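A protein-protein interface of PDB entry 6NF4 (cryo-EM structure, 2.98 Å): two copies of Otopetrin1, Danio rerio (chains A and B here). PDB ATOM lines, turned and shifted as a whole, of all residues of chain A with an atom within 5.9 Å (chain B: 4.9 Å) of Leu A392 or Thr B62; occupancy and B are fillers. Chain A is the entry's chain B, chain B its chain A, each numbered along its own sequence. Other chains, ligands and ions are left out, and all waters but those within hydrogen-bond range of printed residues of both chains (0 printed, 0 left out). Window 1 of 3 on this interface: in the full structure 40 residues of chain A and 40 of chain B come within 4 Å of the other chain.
O of Gln B59 is in hydrogen-bond range of ND2 of Asn B63, 2.5 Å away.
The backbone carbonyl oxygen (O) of Ala B58 sits at hydrogen-bond distance from the side-chain hydroxyl (OG1) of Thr B62, 2.7 Å away.
Of the printed residues of chain B, Leu A392 touches Thr B62 (3.6 Å) and Leu B66 (3.8 Å).
Of the printed residues of chain A, Thr B62 touches Leu A392 (3.6 Å) and Trp A395 (3.8 Å).
Printed residues of chain B within 4 Å of Trp A395: Gln B59, Thr B62, Asn B63 and Leu B66.
Of the printed residues of chain B, Leu A388 touches Gln B59.
Phe B203 touches none of the printed residues of chain A.
Ser A391 touches none of the printed residues of chain B.
The nearest printed residue of chain B that does not touch Leu A392 is Leu B65 (6.6 Å).
The nearest residue of chain A that does not touch Thr B62 is Leu A388 (5.0 Å).
The nearest printed residue of chain B that does not touch Leu A388 is Ala B58 (4.3 Å).
Hydrophobic or aromatic side chains of chain A that line the printed part of chain B: Leu A388, Leu A392 and Trp A395.
Of the 11 printed residues of chain B, 4 touch a printed residue of chain A.
Among the printed residues, 7 pairs touch across the chains.
No position is printed for both chains.
Of the 7 pairs that touch across the chains among the printed residues, none has its exchanged pair printed and touching as well.
Among the printed residues, pairs that only touch across the chains: Trp A395 with Asn B63 (3.5 Å), Leu A392 with Thr B62 (3.6 Å), Leu A388 with Gln B59 (3.7 Å), Trp A395 with Leu B66 (3.7 Å), Leu A392 with Leu B66 (3.8 Å), Trp A395 with Thr B62 (3.8 Å) and Trp A395 with Gln B59 (3.9 Å).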
ATOM      1  N   LEU A 387      -4.557 -11.857 -14.592  1.00  0.00           N
ATOM      2  CA  LEU A 387      -5.344 -10.664 -14.281  1.00  0.00           C
ATOM      3  C   LEU A 387      -4.468  -9.427 -14.105  1.00  0.00           C
ATOM      4  O   LEU A 387      -4.841  -8.335 -14.548  1.00  0.00           O
ATOM      5  CB  LEU A 387      -6.191 -10.894 -13.036  1.00  0.00           C
ATOM      6  CG  LEU A 387      -7.437 -11.751 -13.235  1.00  0.00           C
ATOM      7  CD1 LEU A 387      -8.027 -12.127 -11.910  1.00  0.00           C
ATOM      8  CD2 LEU A 387      -8.454 -11.007 -14.056  1.00  0.00           C
ATOM      9  N   LEU A 388      -3.295  -9.573 -13.485  1.00  0.00           N
ATOM     10  CA  LEU A 388      -2.402  -8.425 -13.331  1.00  0.00           C
ATOM     11  C   LEU A 388      -1.824  -7.967 -14.665  1.00  0.00           C
ATOM     12  O   LEU A 388      -1.741  -6.756 -14.929  1.00  0.00           O
ATOM     13  CB  LEU A 388      -1.274  -8.756 -12.364  1.00  0.00           C
ATOM     14  CG  LEU A 388      -1.605  -8.715 -10.882  1.00  0.00           C
ATOM     15  CD1 LEU A 388      -0.489  -9.342 -10.090  1.00  0.00           C
ATOM     16  CD2 LEU A 388      -1.770  -7.282 -10.488  1.00  0.00           C
ATOM     17  N   ALA A 389      -1.428  -8.916 -15.520  1.00  0.00           N
ATOM     18  CA  ALA A 389      -0.905  -8.567 -16.833  1.00  0.00           C
ATOM     19  C   ALA A 389      -1.963  -7.899 -17.695  1.00  0.00           C
ATOM     20  O   ALA A 389      -1.650  -7.006 -18.487  1.00  0.00           O
ATOM     21  CB  ALA A 389      -0.363  -9.813 -17.520  1.00  0.00           C
ATOM     22  N   SER A 390      -3.222  -8.316 -17.561  1.00  0.00           N
ATOM     23  CA  SER A 390      -4.289  -7.638 -18.285  1.00  0.00           C
ATOM     24  C   SER A 390      -4.558  -6.247 -17.721  1.00  0.00           C
ATOM     25  O   SER A 390      -4.878  -5.318 -18.469  1.00  0.00           O
ATOM     26  CB  SER A 390      -5.546  -8.490 -18.242  1.00  0.00           C
ATOM     27  OG  SER A 390      -5.253  -9.812 -18.635  1.00  0.00           O
ATOM     28  N   SER A 391      -4.452  -6.085 -16.399  1.00  0.00           N
ATOM     29  CA  SER A 391      -4.723  -4.796 -15.770  1.00  0.00           C
ATOM     30  C   SER A 391      -3.650  -3.751 -16.050  1.00  0.00           C
ATOM     31  O   SER A 391      -3.918  -2.554 -15.865  1.00  0.00           O
ATOM     32  CB  SER A 391      -4.866  -4.986 -14.270  1.00  0.00           C
ATOM     33  OG  SER A 391      -5.937  -5.853 -13.975  1.00  0.00           O
ATOM     34  N   LEU A 392      -2.443  -4.187 -16.446  1.00  0.00           N
ATOM     35  CA  LEU A 392      -1.311  -3.277 -16.663  1.00  0.00           C
ATOM     36  C   LEU A 392      -1.586  -2.161 -17.662  1.00  0.00           C
ATOM     37  O   LEU A 392      -1.185  -1.017 -17.424  1.00  0.00           O
ATOM     38  CB  LEU A 392      -0.101  -4.057 -17.154  1.00  0.00           C
ATOM     39  CG  LEU A 392       0.696  -4.857 -16.149  1.00  0.00           C
ATOM     40  CD1 LEU A 392       1.617  -5.755 -16.889  1.00  0.00           C
ATOM     41  CD2 LEU A 392       1.492  -3.884 -15.378  1.00  0.00           C
ATOM     42  N   GLY A 393      -2.249  -2.464 -18.772  1.00  0.00           N
ATOM     43  CA  GLY A 393      -2.475  -1.491 -19.823  1.00  0.00           C
ATOM     44  C   GLY A 393      -3.356  -0.339 -19.400  1.00  0.00           C
ATOM     45  O   GLY A 393      -3.012   0.835 -19.584  1.00  0.00           O
ATOM     46  N   SER A 394      -4.494  -0.678 -18.804  1.00  0.00           N
ATOM     47  CA  SER A 394      -5.400   0.349 -18.318  1.00  0.00           C
ATOM     48  C   SER A 394      -4.839   1.101 -17.126  1.00  0.00           C
ATOM     49  O   SER A 394      -5.139   2.288 -16.968  1.00  0.00           O
ATOM     50  CB  SER A 394      -6.727  -0.265 -17.948  1.00  0.00           C
ATOM     51  OG  SER A 394      -7.506   0.666 -17.226  1.00  0.00           O
ATOM     52  N   TRP A 395      -4.032   0.450 -16.280  1.00  0.00           N
ATOM     53  CA  TRP A 395      -3.379   1.188 -15.203  1.00  0.00           C
ATOM     54  C   TRP A 395      -2.384   2.204 -15.747  1.00  0.00           C
ATOM     55  O   TRP A 395      -2.296   3.324 -15.233  1.00  0.00           O
ATOM     56  CB  TRP A 395      -2.678   0.236 -14.247  1.00  0.00           C
ATOM     57  CG  TRP A 395      -3.591  -0.489 -13.340  1.00  0.00           C
ATOM     58  CD1 TRP A 395      -4.874  -0.170 -13.047  1.00  0.00           C
ATOM     59  CD2 TRP A 395      -3.280  -1.652 -12.577  1.00  0.00           C
ATOM     60  NE1 TRP A 395      -5.393  -1.072 -12.158  1.00  0.00           N
ATOM     61  CE2 TRP A 395      -4.428  -1.993 -11.854  1.00  0.00           C
ATOM     62  CE3 TRP A 395      -2.141  -2.445 -12.446  1.00  0.00           C
ATOM     63  CZ2 TRP A 395      -4.472  -3.088 -11.014  1.00  0.00           C
ATOM     64  CZ3 TRP A 395      -2.188  -3.528 -11.613  1.00  0.00           C
ATOM     65  CH2 TRP A 395      -3.342  -3.841 -10.906  1.00  0.00           C
ATOM     66  N   LEU A 396      -1.641   1.842 -16.795  1.00  0.00           N
ATOM     67  CA  LEU A 396      -0.713   2.782 -17.420  1.00  0.00           C
ATOM     68  C   LEU A 396      -1.449   3.955 -18.055  1.00  0.00           C
ATOM     69  O   LEU A 396      -1.029   5.111 -17.920  1.00  0.00           O
ATOM     70  CB  LEU A 396       0.132   2.058 -18.462  1.00  0.00           C
ATOM     71  CG  LEU A 396       1.104   2.898 -19.282  1.00  0.00           C
ATOM     72  CD1 LEU A 396       2.137   3.548 -18.400  1.00  0.00           C
ATOM     73  CD2 LEU A 396       1.762   2.041 -20.330  1.00  0.00           C
ATOM     74  N   MET A 397      -2.556   3.669 -18.744  1.00  0.00           N
ATOM     75  CA  MET A 397      -3.378   4.714 -19.354  1.00  0.00           C
ATOM     76  C   MET A 397      -3.951   5.668 -18.308  1.00  0.00           C
ATOM     77  O   MET A 397      -3.922   6.895 -18.480  1.00  0.00           O
ATOM     78  CB  MET A 397      -4.492   4.055 -20.163  1.00  0.00           C
ATOM     79  CG  MET A 397      -5.457   4.983 -20.842  1.00  0.00           C
ATOM     80  SD  MET A 397      -6.731   4.038 -21.698  1.00  0.00           S
ATOM     81  CE  MET A 397      -7.730   3.452 -20.343  1.00  0.00           C
ATOM     82  N   LEU A 568      -5.543  -4.795 -24.399  1.00  0.00           N
ATOM     83  CA  LEU A 568      -5.390  -5.446 -23.101  1.00  0.00           C
ATOM     84  C   LEU A 568      -6.629  -5.260 -22.243  1.00  0.00           C
ATOM     85  O   LEU A 568      -7.007  -6.168 -21.498  1.00  0.00           O
ATOM     86  CB  LEU A 568      -4.164  -4.915 -22.366  1.00  0.00           C
ATOM     87  CG  LEU A 568      -2.794  -5.474 -22.716  1.00  0.00           C
ATOM     88  CD1 LEU A 568      -1.721  -4.665 -22.044  1.00  0.00           C
ATOM     89  CD2 LEU A 568      -2.710  -6.904 -22.273  1.00  0.00           C
ATOM     90  N   SER B  57      -0.244  -6.057  -2.223  1.00  0.00           N
ATOM     91  CA  SER B  57       1.099  -5.503  -2.312  1.00  0.00           C
ATOM     92  C   SER B  57       1.613  -5.531  -3.742  1.00  0.00           C
ATOM     93  O   SER B  57       2.274  -4.587  -4.184  1.00  0.00           O
ATOM     94  CB  SER B  57       2.037  -6.266  -1.390  1.00  0.00           C
ATOM     95  OG  SER B  57       2.193  -7.592  -1.843  1.00  0.00           O
ATOM     96  N   ALA B  58       1.294  -6.593  -4.489  1.00  0.00           N
ATOM     97  CA  ALA B  58       1.672  -6.667  -5.895  1.00  0.00           C
ATOM     98  C   ALA B  58       0.999  -5.578  -6.718  1.00  0.00           C
ATOM     99  O   ALA B  58       1.648  -4.934  -7.548  1.00  0.00           O
ATOM    100  CB  ALA B  58       1.319  -8.041  -6.450  1.00  0.00           C
ATOM    101  N   GLN B  59      -0.291  -5.331  -6.471  1.00  0.00           N
ATOM    102  CA  GLN B  59      -1.002  -4.283  -7.200  1.00  0.00           C
ATOM    103  C   GLN B  59      -0.497  -2.896  -6.831  1.00  0.00           C
ATOM    104  O   GLN B  59      -0.382  -2.026  -7.701  1.00  0.00           O
ATOM    105  CB  GLN B  59      -2.493  -4.374  -6.927  1.00  0.00           C
ATOM    106  CG  GLN B  59      -3.122  -5.600  -7.479  1.00  0.00           C
ATOM    107  CD  GLN B  59      -4.560  -5.698  -7.110  1.00  0.00           C
ATOM    108  OE1 GLN B  59      -5.044  -4.970  -6.255  1.00  0.00           O
ATOM    109  NE2 GLN B  59      -5.252  -6.627  -7.723  1.00  0.00           N
ATOM    110  N   TYR B  60      -0.196  -2.676  -5.549  1.00  0.00           N
ATOM    111  CA  TYR B  60       0.345  -1.398  -5.100  1.00  0.00           C
ATOM    112  C   TYR B  60       1.699  -1.110  -5.729  1.00  0.00           C
ATOM    113  O   TYR B  60       1.930  -0.012  -6.246  1.00  0.00           O
ATOM    114  CB  TYR B  60       0.446  -1.390  -3.577  1.00  0.00           C
ATOM    115  CG  TYR B  60       1.388  -0.352  -3.036  1.00  0.00           C
ATOM    116  CD1 TYR B  60       1.054   0.988  -3.051  1.00  0.00           C
ATOM    117  CD2 TYR B  60       2.605  -0.718  -2.489  1.00  0.00           C
ATOM    118  CE1 TYR B  60       1.914   1.935  -2.557  1.00  0.00           C
ATOM    119  CE2 TYR B  60       3.467   0.218  -1.996  1.00  0.00           C
ATOM    120  CZ  TYR B  60       3.115   1.540  -2.030  1.00  0.00           C
ATOM    121  OH  TYR B  60       3.974   2.480  -1.533  1.00  0.00           O
ATOM    122  N   GLY B  61       2.611  -2.083  -5.690  1.00  0.00           N
ATOM    123  CA  GLY B  61       3.925  -1.877  -6.276  1.00  0.00           C
ATOM    124  C   GLY B  61       3.888  -1.720  -7.781  1.00  0.00           C
ATOM    125  O   GLY B  61       4.637  -0.922  -8.350  1.00  0.00           O
ATOM    126  N   THR B  62       3.013  -2.476  -8.444  1.00  0.00           N
ATOM    127  CA  THR B  62       2.839  -2.349  -9.884  1.00  0.00           C
ATOM    128  C   THR B  62       2.315  -0.969 -10.266  1.00  0.00           C
ATOM    129  O   THR B  62       2.808  -0.347 -11.212  1.00  0.00           O
ATOM    130  CB  THR B  62       1.905  -3.451 -10.357  1.00  0.00           C
ATOM    131  OG1 THR B  62       2.524  -4.718 -10.126  1.00  0.00           O
ATOM    132  CG2 THR B  62       1.618  -3.315 -11.794  1.00  0.00           C
ATOM    133  N   ASN B  63       1.348  -0.446  -9.506  1.00  0.00           N
ATOM    134  CA  ASN B  63       0.863   0.907  -9.757  1.00  0.00           C
ATOM    135  C   ASN B  63       1.911   1.962  -9.444  1.00  0.00           C
ATOM    136  O   ASN B  63       1.938   3.012 -10.089  1.00  0.00           O
ATOM    137  CB  ASN B  63      -0.388   1.174  -8.939  1.00  0.00           C
ATOM    138  CG  ASN B  63      -1.586   0.490  -9.498  1.00  0.00           C
ATOM    139  OD1 ASN B  63      -2.130   0.910 -10.510  1.00  0.00           O
ATOM    140  ND2 ASN B  63      -2.010  -0.575  -8.850  1.00  0.00           N
ATOM    141  N   LEU B  64       2.779   1.696  -8.470  1.00  0.00           N
ATOM    142  CA  LEU B  64       3.868   2.614  -8.157  1.00  0.00           C
ATOM    143  C   LEU B  64       4.854   2.706  -9.318  1.00  0.00           C
ATOM    144  O   LEU B  64       5.274   3.803  -9.721  1.00  0.00           O
ATOM    145  CB  LEU B  64       4.560   2.132  -6.890  1.00  0.00           C
ATOM    146  CG  LEU B  64       5.571   3.044  -6.243  1.00  0.00           C
ATOM    147  CD1 LEU B  64       4.806   4.253  -5.793  1.00  0.00           C
ATOM    148  CD2 LEU B  64       6.208   2.336  -5.082  1.00  0.00           C
ATOM    149  N   LEU B  65       5.203   1.549  -9.886  1.00  0.00           N
ATOM    150  CA  LEU B  65       6.061   1.502 -11.066  1.00  0.00           C
ATOM    151  C   LEU B  65       5.423   2.204 -12.256  1.00  0.00           C
ATOM    152  O   LEU B  65       6.088   2.961 -12.967  1.00  0.00           O
ATOM    153  CB  LEU B  65       6.378   0.055 -11.422  1.00  0.00           C
ATOM    154  CG  LEU B  65       7.233  -0.148 -12.667  1.00  0.00           C
ATOM    155  CD1 LEU B  65       8.626   0.395 -12.442  1.00  0.00           C
ATOM    156  CD2 LEU B  65       7.272  -1.604 -13.049  1.00  0.00           C
ATOM    157  N   LEU B  66       4.133   1.958 -12.497  1.00  0.00           N
ATOM    158  CA  LEU B  66       3.475   2.555 -13.658  1.00  0.00           C
ATOM    159  C   LEU B  66       3.281   4.057 -13.492  1.00  0.00           C
ATOM    160  O   LEU B  66       3.288   4.797 -14.481  1.00  0.00           O
ATOM    161  CB  LEU B  66       2.150   1.861 -13.926  1.00  0.00           C
ATOM    162  CG  LEU B  66       2.339   0.427 -14.402  1.00  0.00           C
ATOM    163  CD1 LEU B  66       1.016  -0.261 -14.469  1.00  0.00           C
ATOM    164  CD2 LEU B  66       3.016   0.396 -15.744  1.00  0.00           C
ATOM    165  N   PHE B 203      10.306  -1.594  -5.856  1.00  0.00           N
ATOM    166  CA  PHE B 203       9.964  -0.692  -6.945  1.00  0.00           C
ATOM    167  C   PHE B 203      10.587   0.685  -6.772  1.00  0.00           C
ATOM    168  O   PHE B 203      10.800   1.382  -7.770  1.00  0.00           O
ATOM    169  CB  PHE B 203       8.454  -0.647  -7.109  1.00  0.00           C
ATOM    170  CG  PHE B 203       7.906  -1.906  -7.703  1.00  0.00           C
ATOM    171  CD1 PHE B 203       7.297  -2.853  -6.911  1.00  0.00           C
ATOM    172  CD2 PHE B 203       8.054  -2.165  -9.048  1.00  0.00           C
ATOM    173  CE1 PHE B 203       6.811  -4.019  -7.458  1.00  0.00           C
ATOM    174  CE2 PHE B 203       7.575  -3.328  -9.596  1.00  0.00           C
ATOM    175  CZ  PHE B 203       6.953  -4.253  -8.800  1.00  0.00           C
